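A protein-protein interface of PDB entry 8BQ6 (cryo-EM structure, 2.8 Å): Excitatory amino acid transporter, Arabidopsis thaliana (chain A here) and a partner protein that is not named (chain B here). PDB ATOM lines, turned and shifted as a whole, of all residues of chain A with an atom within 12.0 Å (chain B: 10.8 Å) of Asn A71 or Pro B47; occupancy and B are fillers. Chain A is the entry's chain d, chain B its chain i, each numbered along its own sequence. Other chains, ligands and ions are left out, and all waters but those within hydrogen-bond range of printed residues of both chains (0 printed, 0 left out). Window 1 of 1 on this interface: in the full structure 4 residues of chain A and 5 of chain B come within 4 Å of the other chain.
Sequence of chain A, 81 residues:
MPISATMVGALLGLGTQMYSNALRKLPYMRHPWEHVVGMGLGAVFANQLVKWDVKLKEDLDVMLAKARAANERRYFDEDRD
Of the 15 printed residues of chain A, 4 touch a printed residue of chain B. Of the 16 printed residues of chain B, 5 touch a printed residue of chain A. Hydrophobic or aromatic side chains of chain B within 4 Å of the printed part of chain A: Met B43, Leu B46, Pro B47, Tyr B51 and Phe B56. Among the printed residues, no Asp or Glu carboxylate lies within 4 Å of a Lys or Arg side-chain nitrogen of the other chain.
Met A63 touches none of the printed residues of chain B. Of the printed residues of chain B, Leu A64 touches Met B43 and Leu B46. Ala A67 touches none of the printed residues of chain B. No residue of chain B comes within 4 Å of Ala A69. Ala A70 touches just these residues of chain B: Tyr B51 (3.8 Å) and Phe B56 (3.9 Å). Of chain B, only Pro B47 comes within 4 Å of Asn A71. Arg A74 touches two residues of chain B. Of the printed residues of chain A, Met B43 touches Leu A64 (3.8 Å). No residue of chain A comes within 4 Å of Ala B45. Printed residues of chain A within 4 Å of Leu B46: Leu A64. Ile B48 touches none of the printed residues of chain A. No residue of chain A comes within 4 Å of Arg B49. No residue of chain A comes within 4 Å of Pro B50. Printed residues of chain A within 4 Å of Tyr B51: Ala A70 (3.8 Å) and Arg A74 (3.5 Å). Of the printed residues of chain A, Phe B56 touches Ala A70 (3.9 Å). The nearest residue of chain B that does not touch Asn A71 is Leu B46 (4.9 Å). The nearest residue of chain A that does not touch Pro B47 is Ala A67 (6.3 Å).
O of Leu A64 sits close to NH1 of Arg A68, at 3.4 Å. The guanidinium group (NH1) of Arg A74 is in hydrogen-bond range of the side-chain amide oxygen (OD1) of Asn A71.
Among the printed residues, pairs that only touch across the chains: Leu A64 with Met B43, Leu A64 with Leu B46, Ala A70 with Tyr B51, Ala A70 with Phe B56, Asn A71 with Pro B47, Arg A74 with Pro B47 and Arg A74 with Tyr B51.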
ATOM      1  N   VAL A  62     -12.362  -7.038 -29.215  1.00  0.00           N
ATOM      2  CA  VAL A  62     -10.889  -6.785 -29.202  1.00  0.00           C
ATOM      3  C   VAL A  62     -10.502  -6.160 -27.856  1.00  0.00           C
ATOM      4  O   VAL A  62      -9.537  -6.647 -27.237  1.00  0.00           O
ATOM      5  CB  VAL A  62     -10.465  -5.891 -30.385  1.00  0.00           C
ATOM      6  CG1 VAL A  62      -8.975  -5.586 -30.374  1.00  0.00           C
ATOM      7  CG2 VAL A  62     -10.873  -6.491 -31.720  1.00  0.00           C
ATOM      8  N   MET A  63     -11.233  -5.129 -27.422  1.00  0.00           N
ATOM      9  CA  MET A  63     -10.936  -4.448 -26.133  1.00  0.00           C
ATOM     10  C   MET A  63     -11.057  -5.443 -24.972  1.00  0.00           C
ATOM     11  O   MET A  63     -10.187  -5.405 -24.084  1.00  0.00           O
ATOM     12  CB  MET A  63     -11.900  -3.281 -25.904  1.00  0.00           C
ATOM     13  CG  MET A  63     -11.696  -2.137 -26.874  1.00  0.00           C
ATOM     14  SD  MET A  63     -12.902  -0.814 -26.634  1.00  0.00           S
ATOM     15  CE  MET A  63     -12.316  -0.115 -25.091  1.00  0.00           C
ATOM     16  N   LEU A  64     -12.092  -6.293 -24.976  1.00  0.00           N
ATOM     17  CA  LEU A  64     -12.290  -7.241 -23.887  1.00  0.00           C
ATOM     18  C   LEU A  64     -11.203  -8.309 -23.892  1.00  0.00           C
ATOM     19  O   LEU A  64     -10.757  -8.759 -22.829  1.00  0.00           O
ATOM     20  CB  LEU A  64     -13.675  -7.874 -23.983  1.00  0.00           C
ATOM     21  CG  LEU A  64     -14.684  -7.346 -22.969  1.00  0.00           C
ATOM     22  CD1 LEU A  64     -16.083  -7.806 -23.323  1.00  0.00           C
ATOM     23  CD2 LEU A  64     -14.293  -7.827 -21.592  1.00  0.00           C
ATOM     24  N   ALA A  65     -10.750  -8.712 -25.082  1.00  0.00           N
ATOM     25  CA  ALA A  65      -9.638  -9.650 -25.176  1.00  0.00           C
ATOM     26  C   ALA A  65      -8.392  -9.076 -24.517  1.00  0.00           C
ATOM     27  O   ALA A  65      -7.718  -9.755 -23.730  1.00  0.00           O
ATOM     28  CB  ALA A  65      -9.365  -9.986 -26.643  1.00  0.00           C
ATOM     29  N   LYS A  66      -8.079  -7.816 -24.821  1.00  0.00           N
ATOM     30  CA  LYS A  66      -6.905  -7.185 -24.223  1.00  0.00           C
ATOM     31  C   LYS A  66      -7.050  -7.048 -22.711  1.00  0.00           C
ATOM     32  O   LYS A  66      -6.090  -7.291 -21.967  1.00  0.00           O
ATOM     33  CB  LYS A  66      -6.654  -5.827 -24.870  1.00  0.00           C
ATOM     34  CG  LYS A  66      -6.172  -5.939 -26.302  1.00  0.00           C
ATOM     35  CD  LYS A  66      -6.010  -4.583 -26.962  1.00  0.00           C
ATOM     36  CE  LYS A  66      -5.576  -4.750 -28.412  1.00  0.00           C
ATOM     37  NZ  LYS A  66      -5.455  -3.452 -29.137  1.00  0.00           N
ATOM     38  N   ALA A  67      -8.233  -6.656 -22.233  1.00  0.00           N
ATOM     39  CA  ALA A  67      -8.427  -6.536 -20.792  1.00  0.00           C
ATOM     40  C   ALA A  67      -8.231  -7.878 -20.099  1.00  0.00           C
ATOM     41  O   ALA A  67      -7.568  -7.955 -19.056  1.00  0.00           O
ATOM     42  CB  ALA A  67      -9.813  -5.974 -20.481  1.00  0.00           C
ATOM     43  N   ARG A  68      -8.783  -8.952 -20.671  1.00  0.00           N
ATOM     44  CA  ARG A  68      -8.612 -10.265 -20.056  1.00  0.00           C
ATOM     45  C   ARG A  68      -7.160 -10.718 -20.099  1.00  0.00           C
ATOM     46  O   ARG A  68      -6.689 -11.381 -19.170  1.00  0.00           O
ATOM     47  CB  ARG A  68      -9.511 -11.304 -20.721  1.00  0.00           C
ATOM     48  CG  ARG A  68     -10.989 -11.004 -20.654  1.00  0.00           C
ATOM     49  CD  ARG A  68     -11.784 -12.275 -20.899  1.00  0.00           C
ATOM     50  NE  ARG A  68     -13.104 -12.006 -21.454  1.00  0.00           N
ATOM     51  CZ  ARG A  68     -13.335 -11.727 -22.729  1.00  0.00           C
ATOM     52  NH1 ARG A  68     -12.350 -11.659 -23.610  1.00  0.00           N
ATOM     53  NH2 ARG A  68     -14.584 -11.517 -23.131  1.00  0.00           N
ATOM     54  N   ALA A  69      -6.434 -10.390 -21.169  1.00  0.00           N
ATOM     55  CA  ALA A  69      -5.014 -10.736 -21.203  1.00  0.00           C
ATOM     56  C   ALA A  69      -4.246  -9.997 -20.112  1.00  0.00           C
ATOM     57  O   ALA A  69      -3.416 -10.592 -19.408  1.00  0.00           O
ATOM     58  CB  ALA A  69      -4.427 -10.428 -22.579  1.00  0.00           C
ATOM     59  N   ALA A  70      -4.529  -8.704 -19.944  1.00  0.00           N
ATOM     60  CA  ALA A  70      -3.864  -7.930 -18.902  1.00  0.00           C
ATOM     61  C   ALA A  70      -4.186  -8.486 -17.524  1.00  0.00           C
ATOM     62  O   ALA A  70      -3.333  -8.485 -16.628  1.00  0.00           O
ATOM     63  CB  ALA A  70      -4.271  -6.461 -18.990  1.00  0.00           C
ATOM     64  N   ASN A  71      -5.417  -8.959 -17.335  1.00  0.00           N
ATOM     65  CA  ASN A  71      -5.799  -9.506 -16.038  1.00  0.00           C
ATOM     66  C   ASN A  71      -5.155 -10.866 -15.791  1.00  0.00           C
ATOM     67  O   ASN A  71      -4.721 -11.158 -14.670  1.00  0.00           O
ATOM     68  CB  ASN A  71      -7.316  -9.606 -15.938  1.00  0.00           C
ATOM     69  CG  ASN A  71      -7.774  -9.967 -14.546  1.00  0.00           C
ATOM     70  OD1 ASN A  71      -7.388  -9.321 -13.572  1.00  0.00           O
ATOM     71  ND2 ASN A  71      -8.586 -11.011 -14.439  1.00  0.00           N
ATOM     72  N   GLU A  72      -5.098 -11.721 -16.816  1.00  0.00           N
ATOM     73  CA  GLU A  72      -4.446 -13.017 -16.674  1.00  0.00           C
ATOM     74  C   GLU A  72      -2.948 -12.879 -16.458  1.00  0.00           C
ATOM     75  O   GLU A  72      -2.334 -13.780 -15.877  1.00  0.00           O
ATOM     76  CB  GLU A  72      -4.713 -13.893 -17.902  1.00  0.00           C
ATOM     77  CG  GLU A  72      -6.167 -14.318 -18.054  1.00  0.00           C
ATOM     78  CD  GLU A  72      -6.435 -15.096 -19.333  1.00  0.00           C
ATOM     79  OE1 GLU A  72      -5.496 -15.288 -20.134  1.00  0.00           O
ATOM     80  OE2 GLU A  72      -7.599 -15.496 -19.549  1.00  0.00           O
ATOM     81  N   ARG A  73      -2.351 -11.769 -16.901  1.00  0.00           N
ATOM     82  CA  ARG A  73      -0.939 -11.540 -16.615  1.00  0.00           C
ATOM     83  C   ARG A  73      -0.653 -11.535 -15.119  1.00  0.00           C
ATOM     84  O   ARG A  73       0.490 -11.782 -14.720  1.00  0.00           O
ATOM     85  CB  ARG A  73      -0.475 -10.216 -17.224  1.00  0.00           C
ATOM     86  CG  ARG A  73      -0.192 -10.276 -18.713  1.00  0.00           C
ATOM     87  CD  ARG A  73       0.820 -11.359 -19.026  1.00  0.00           C
ATOM     88  NE  ARG A  73       2.176 -10.995 -18.631  1.00  0.00           N
ATOM     89  CZ  ARG A  73       3.002 -10.264 -19.367  1.00  0.00           C
ATOM     90  NH1 ARG A  73       2.633  -9.773 -20.539  1.00  0.00           N
ATOM     91  NH2 ARG A  73       4.230 -10.024 -18.918  1.00  0.00           N
ATOM     92  N   ARG A  74      -1.664 -11.272 -14.286  1.00  0.00           N
ATOM     93  CA  ARG A  74      -1.438 -11.199 -12.846  1.00  0.00           C
ATOM     94  C   ARG A  74      -0.929 -12.523 -12.293  1.00  0.00           C
ATOM     95  O   ARG A  74      -0.026 -12.544 -11.447  1.00  0.00           O
ATOM     96  CB  ARG A  74      -2.719 -10.786 -12.124  1.00  0.00           C
ATOM     97  CG  ARG A  74      -2.460 -10.242 -10.727  1.00  0.00           C
ATOM     98  CD  ARG A  74      -3.737 -10.071  -9.938  1.00  0.00           C
ATOM     99  NE  ARG A  74      -4.448  -8.862 -10.330  1.00  0.00           N
ATOM    100  CZ  ARG A  74      -5.598  -8.856 -10.988  1.00  0.00           C
ATOM    101  NH1 ARG A  74      -6.207  -9.982 -11.324  1.00  0.00           N
ATOM    102  NH2 ARG A  74      -6.155  -7.694 -11.314  1.00  0.00           N
ATOM    103  N   TYR A  75      -1.485 -13.636 -12.765  1.00  0.00           N
ATOM    104  CA  TYR A  75      -1.175 -14.955 -12.234  1.00  0.00           C
ATOM    105  C   TYR A  75       0.055 -15.585 -12.876  1.00  0.00           C
ATOM    106  O   TYR A  75       0.230 -16.807 -12.786  1.00  0.00           O
ATOM    107  CB  TYR A  75      -2.388 -15.873 -12.396  1.00  0.00           C
ATOM    108  CG  TYR A  75      -3.652 -15.306 -11.790  1.00  0.00           C
ATOM    109  CD1 TYR A  75      -3.618 -14.621 -10.582  1.00  0.00           C
ATOM    110  CD2 TYR A  75      -4.879 -15.459 -12.421  1.00  0.00           C
ATOM    111  CE1 TYR A  75      -4.771 -14.103 -10.020  1.00  0.00           C
ATOM    112  CE2 TYR A  75      -6.038 -14.947 -11.866  1.00  0.00           C
ATOM    113  CZ  TYR A  75      -5.977 -14.270 -10.667  1.00  0.00           C
ATOM    114  OH  TYR A  75      -7.125 -13.756 -10.113  1.00  0.00           O
ATOM    115  N   PHE A  76       0.908 -14.790 -13.510  1.00  0.00           N
ATOM    116  CA  PHE A  76       2.135 -15.307 -14.097  1.00  0.00           C
ATOM    117  C   PHE A  76       3.278 -15.228 -13.092  1.00  0.00           C
ATOM    118  O   PHE A  76       3.221 -14.453 -12.139  1.00  0.00           O
ATOM    119  CB  PHE A  76       2.488 -14.537 -15.367  1.00  0.00           C
ATOM    120  CG  PHE A  76       2.081 -15.240 -16.626  1.00  0.00           C
ATOM    121  CD1 PHE A  76       2.932 -16.145 -17.236  1.00  0.00           C
ATOM    122  CD2 PHE A  76       0.836 -15.013 -17.188  1.00  0.00           C
ATOM    123  CE1 PHE A  76       2.554 -16.801 -18.390  1.00  0.00           C
ATOM    124  CE2 PHE A  76       0.452 -15.666 -18.341  1.00  0.00           C
ATOM    125  CZ  PHE A  76       1.311 -16.562 -18.943  1.00  0.00           C
ATOM    126  N   LYS B  41     -20.738 -13.957 -15.365  1.00  0.00           N
ATOM    127  CA  LYS B  41     -20.290 -13.574 -14.033  1.00  0.00           C
ATOM    128  C   LYS B  41     -18.787 -13.343 -13.976  1.00  0.00           C
ATOM    129  O   LYS B  41     -18.302 -12.727 -13.020  1.00  0.00           O
ATOM    130  CB  LYS B  41     -20.710 -14.633 -13.017  1.00  0.00           C
ATOM    131  CG  LYS B  41     -21.974 -14.273 -12.260  1.00  0.00           C
ATOM    132  CD  LYS B  41     -22.129 -15.123 -11.019  1.00  0.00           C
ATOM    133  CE  LYS B  41     -22.939 -16.370 -11.317  1.00  0.00           C
ATOM    134  NZ  LYS B  41     -24.319 -16.036 -11.746  1.00  0.00           N
ATOM    135  N   GLU B  42     -18.036 -13.825 -14.971  1.00  0.00           N
ATOM    136  CA  GLU B  42     -16.631 -13.449 -15.070  1.00  0.00           C
ATOM    137  C   GLU B  42     -16.479 -11.964 -15.385  1.00  0.00           C
ATOM    138  O   GLU B  42     -15.540 -11.322 -14.900  1.00  0.00           O
ATOM    139  CB  GLU B  42     -15.923 -14.291 -16.139  1.00  0.00           C
ATOM    140  CG  GLU B  42     -15.940 -15.808 -15.917  1.00  0.00           C
ATOM    141  CD  GLU B  42     -14.653 -16.343 -15.300  1.00  0.00           C
ATOM    142  OE1 GLU B  42     -13.788 -15.531 -14.914  1.00  0.00           O
ATOM    143  OE2 GLU B  42     -14.502 -17.580 -15.208  1.00  0.00           O
ATOM    144  N   MET B  43     -17.393 -11.403 -16.186  1.00  0.00           N
ATOM    145  CA  MET B  43     -17.251 -10.019 -16.634  1.00  0.00           C
ATOM    146  C   MET B  43     -17.472  -9.033 -15.494  1.00  0.00           C
ATOM    147  O   MET B  43     -16.766  -8.021 -15.395  1.00  0.00           O
ATOM    148  CB  MET B  43     -18.213  -9.733 -17.791  1.00  0.00           C
ATOM    149  CG  MET B  43     -17.567  -9.014 -18.971  1.00  0.00           C
ATOM    150  SD  MET B  43     -18.711  -8.521 -20.275  1.00  0.00           S
ATOM    151  CE  MET B  43     -18.586  -9.912 -21.394  1.00  0.00           C
ATOM    152  N   TRP B  44     -18.442  -9.309 -14.622  1.00  0.00           N
ATOM    153  CA  TRP B  44     -18.683  -8.436 -13.481  1.00  0.00           C
ATOM    154  C   TRP B  44     -17.520  -8.455 -12.497  1.00  0.00           C
ATOM    155  O   TRP B  44     -17.429  -7.566 -11.643  1.00  0.00           O
ATOM    156  CB  TRP B  44     -19.991  -8.839 -12.789  1.00  0.00           C
ATOM    157  CG  TRP B  44     -21.204  -8.423 -13.579  1.00  0.00           C
ATOM    158  CD1 TRP B  44     -21.247  -7.473 -14.554  1.00  0.00           C
ATOM    159  CD2 TRP B  44     -22.537  -8.954 -13.480  1.00  0.00           C
ATOM    160  NE1 TRP B  44     -22.515  -7.370 -15.064  1.00  0.00           N
ATOM    161  CE2 TRP B  44     -23.327  -8.266 -14.423  1.00  0.00           C
ATOM    162  CE3 TRP B  44     -23.136  -9.936 -12.685  1.00  0.00           C
ATOM    163  CZ2 TRP B  44     -24.684  -8.529 -14.596  1.00  0.00           C
ATOM    164  CZ3 TRP B  44     -24.486 -10.196 -12.859  1.00  0.00           C
ATOM    165  CH2 TRP B  44     -25.244  -9.494 -13.806  1.00  0.00           C
ATOM    166  N   ALA B  45     -16.625  -9.435 -12.606  1.00  0.00           N
ATOM    167  CA  ALA B  45     -15.471  -9.554 -11.727  1.00  0.00           C
ATOM    168  C   ALA B  45     -14.192  -8.969 -12.316  1.00  0.00           C
ATOM    169  O   ALA B  45     -13.160  -8.984 -11.637  1.00  0.00           O
ATOM    170  CB  ALA B  45     -15.237 -11.026 -11.368  1.00  0.00           C
ATOM    171  N   LEU B  46     -14.223  -8.462 -13.545  1.00  0.00           N
ATOM    172  CA  LEU B  46     -13.011  -7.924 -14.156  1.00  0.00           C
ATOM    173  C   LEU B  46     -12.583  -6.656 -13.426  1.00  0.00           C
ATOM    174  O   LEU B  46     -13.413  -5.767 -13.201  1.00  0.00           O
ATOM    175  CB  LEU B  46     -13.230  -7.623 -15.640  1.00  0.00           C
ATOM    176  CG  LEU B  46     -13.445  -8.790 -16.606  1.00  0.00           C
ATOM    177  CD1 LEU B  46     -14.419  -8.387 -17.682  1.00  0.00           C
ATOM    178  CD2 LEU B  46     -12.134  -9.239 -17.231  1.00  0.00           C
ATOM    179  N   PRO B  47     -11.312  -6.532 -13.040  1.00  0.00           N
ATOM    180  CA  PRO B  47     -10.883  -5.337 -12.305  1.00  0.00           C
ATOM    181  C   PRO B  47     -11.085  -4.077 -13.127  1.00  0.00           C
ATOM    182  O   PRO B  47     -10.741  -4.018 -14.311  1.00  0.00           O
ATOM    183  CB  PRO B  47      -9.398  -5.599 -12.038  1.00  0.00           C
ATOM    184  CG  PRO B  47      -8.988  -6.524 -13.129  1.00  0.00           C
ATOM    185  CD  PRO B  47     -10.179  -7.418 -13.351  1.00  0.00           C
ATOM    186  N   ILE B  48     -11.655  -3.061 -12.484  1.00  0.00           N
ATOM    187  CA  ILE B  48     -11.762  -1.763 -13.131  1.00  0.00           C
ATOM    188  C   ILE B  48     -10.377  -1.202 -13.418  1.00  0.00           C
ATOM    189  O   ILE B  48     -10.139  -0.639 -14.492  1.00  0.00           O
ATOM    190  CB  ILE B  48     -12.594  -0.813 -12.257  1.00  0.00           C
ATOM    191  CG1 ILE B  48     -12.541   0.591 -12.831  1.00  0.00           C
ATOM    192  CG2 ILE B  48     -12.089  -0.830 -10.822  1.00  0.00           C
ATOM    193  CD1 ILE B  48     -13.250   1.622 -12.015  1.00  0.00           C
ATOM    194  N   ARG B  49      -9.450  -1.356 -12.475  1.00  0.00           N
ATOM    195  CA  ARG B  49      -8.053  -0.979 -12.616  1.00  0.00           C
ATOM    196  C   ARG B  49      -7.258  -2.239 -12.915  1.00  0.00           C
ATOM    197  O   ARG B  49      -7.084  -3.081 -12.021  1.00  0.00           O
ATOM    198  CB  ARG B  49      -7.553  -0.316 -11.331  1.00  0.00           C
ATOM    199  CG  ARG B  49      -6.069  -0.019 -11.317  1.00  0.00           C
ATOM    200  CD  ARG B  49      -5.450  -0.276  -9.948  1.00  0.00           C
ATOM    201  NE  ARG B  49      -6.300   0.164  -8.848  1.00  0.00           N
ATOM    202  CZ  ARG B  49      -6.701  -0.616  -7.853  1.00  0.00           C
ATOM    203  NH1 ARG B  49      -6.357  -1.893  -7.794  1.00  0.00           N
ATOM    204  NH2 ARG B  49      -7.462  -0.100  -6.891  1.00  0.00           N
ATOM    205  N   PRO B  50      -6.710  -2.483 -14.139  1.00  0.00           N
ATOM    206  CA  PRO B  50      -6.031  -3.771 -14.387  1.00  0.00           C
ATOM    207  C   PRO B  50      -4.671  -3.920 -13.683  1.00  0.00           C
ATOM    208  O   PRO B  50      -4.262  -3.028 -12.952  1.00  0.00           O
ATOM    209  CB  PRO B  50      -5.829  -3.802 -15.909  1.00  0.00           C
ATOM    210  CG  PRO B  50      -5.689  -2.350 -16.280  1.00  0.00           C
ATOM    211  CD  PRO B  50      -6.654  -1.634 -15.362  1.00  0.00           C
ATOM    212  N   TYR B  51      -3.997  -5.045 -13.928  1.00  0.00           N
ATOM    213  CA  TYR B  51      -2.695  -5.293 -13.266  1.00  0.00           C
ATOM    214  C   TYR B  51      -1.630  -4.408 -13.897  1.00  0.00           C
ATOM    215  O   TYR B  51      -1.121  -4.760 -14.984  1.00  0.00           O
ATOM    216  CB  TYR B  51      -2.262  -6.757 -13.360  1.00  0.00           C
ATOM    217  CG  TYR B  51      -1.364  -7.150 -12.217  1.00  0.00           C
ATOM    218  CD1 TYR B  51      -1.680  -6.774 -10.923  1.00  0.00           C
ATOM    219  CD2 TYR B  51      -0.193  -7.859 -12.424  1.00  0.00           C
ATOM    220  CE1 TYR B  51      -0.875  -7.124  -9.853  1.00  0.00           C
ATOM    221  CE2 TYR B  51       0.623  -8.222 -11.365  1.00  0.00           C
ATOM    222  CZ  TYR B  51       0.279  -7.850 -10.078  1.00  0.00           C
ATOM    223  OH  TYR B  51       1.060  -8.195  -9.018  1.00  0.00           O
ATOM    224  N   GLY B  52      -1.312  -3.300 -13.229  1.00  0.00           N
ATOM    225  CA  GLY B  52      -0.276  -2.391 -13.740  1.00  0.00           C
ATOM    226  C   GLY B  52      -0.751  -1.635 -14.959  1.00  0.00           C
ATOM    227  O   GLY B  52      -0.257  -1.931 -16.051  1.00  0.00           O
ATOM    228  N   PHE B  53      -1.699  -0.709 -14.794  1.00  0.00           N
ATOM    229  CA  PHE B  53      -2.072   0.119 -15.973  1.00  0.00           C
ATOM    230  C   PHE B  53      -0.813   0.894 -16.380  1.00  0.00           C
ATOM    231  O   PHE B  53      -0.501   0.871 -17.564  1.00  0.00           O
ATOM    232  CB  PHE B  53      -3.331   0.955 -15.721  1.00  0.00           C
ATOM    233  CG  PHE B  53      -3.194   2.159 -14.826  1.00  0.00           C
ATOM    234  CD1 PHE B  53      -3.474   2.067 -13.474  1.00  0.00           C
ATOM    235  CD2 PHE B  53      -2.837   3.395 -15.344  1.00  0.00           C
ATOM    236  CE1 PHE B  53      -3.367   3.175 -12.652  1.00  0.00           C
ATOM    237  CE2 PHE B  53      -2.718   4.500 -14.518  1.00  0.00           C
ATOM    238  CZ  PHE B  53      -2.987   4.388 -13.175  1.00  0.00           C
ATOM    239  N   TRP B  54      -0.059   1.429 -15.414  1.00  0.00           N
ATOM    240  CA  TRP B  54       1.201   2.184 -15.680  1.00  0.00           C
ATOM    241  C   TRP B  54       2.088   1.449 -16.699  1.00  0.00           C
ATOM    242  O   TRP B  54       2.741   2.143 -17.507  1.00  0.00           O
ATOM    243  CB  TRP B  54       1.929   2.474 -14.355  1.00  0.00           C
ATOM    244  CG  TRP B  54       2.042   1.322 -13.402  1.00  0.00           C
ATOM    245  CD1 TRP B  54       3.070   0.432 -13.311  1.00  0.00           C
ATOM    246  CD2 TRP B  54       1.109   0.952 -12.371  1.00  0.00           C
ATOM    247  NE1 TRP B  54       2.843  -0.468 -12.308  1.00  0.00           N
ATOM    248  CE2 TRP B  54       1.645  -0.176 -11.715  1.00  0.00           C
ATOM    249  CE3 TRP B  54      -0.126   1.452 -11.946  1.00  0.00           C
ATOM    250  CZ2 TRP B  54       0.983  -0.810 -10.666  1.00  0.00           C
ATOM    251  CZ3 TRP B  54      -0.778   0.827 -10.909  1.00  0.00           C
ATOM    252  CH2 TRP B  54      -0.227  -0.286 -10.275  1.00  0.00           C
ATOM    253  N   THR B  55       2.093   0.109 -16.689  1.00  0.00           N
ATOM    254  CA  THR B  55       2.923  -0.712 -17.616  1.00  0.00           C
ATOM    255  C   THR B  55       2.561  -0.477 -19.095  1.00  0.00           C
ATOM    256  O   THR B  55       3.478  -0.607 -19.921  1.00  0.00           O
ATOM    257  CB  THR B  55       2.795  -2.196 -17.235  1.00  0.00           C
ATOM    258  OG1 THR B  55       2.739  -2.318 -15.812  1.00  0.00           O
ATOM    259  CG2 THR B  55       3.929  -3.059 -17.748  1.00  0.00           C
ATOM    260  N   PHE B  56       1.315  -0.108 -19.434  1.00  0.00           N
ATOM    261  CA  PHE B  56       0.866   0.003 -20.857  1.00  0.00           C
ATOM    262  C   PHE B  56       1.587   1.115 -21.623  1.00  0.00           C
ATOM    263  O   PHE B  56       1.972   2.116 -20.986  1.00  0.00           O
ATOM    264  CB  PHE B  56      -0.646   0.220 -20.953  1.00  0.00           C
ATOM    265  CG  PHE B  56      -1.503  -0.806 -20.256  1.00  0.00           C
ATOM    266  CD1 PHE B  56      -1.048  -2.097 -20.032  1.00  0.00           C
ATOM    267  CD2 PHE B  56      -2.783  -0.481 -19.836  1.00  0.00           C
ATOM    268  CE1 PHE B  56      -1.843  -3.030 -19.385  1.00  0.00           C
ATOM    269  CE2 PHE B  56      -3.580  -1.416 -19.195  1.00  0.00           C
ATOM    270  CZ  PHE B  56      -3.107  -2.687 -18.971  1.00  0.00           C
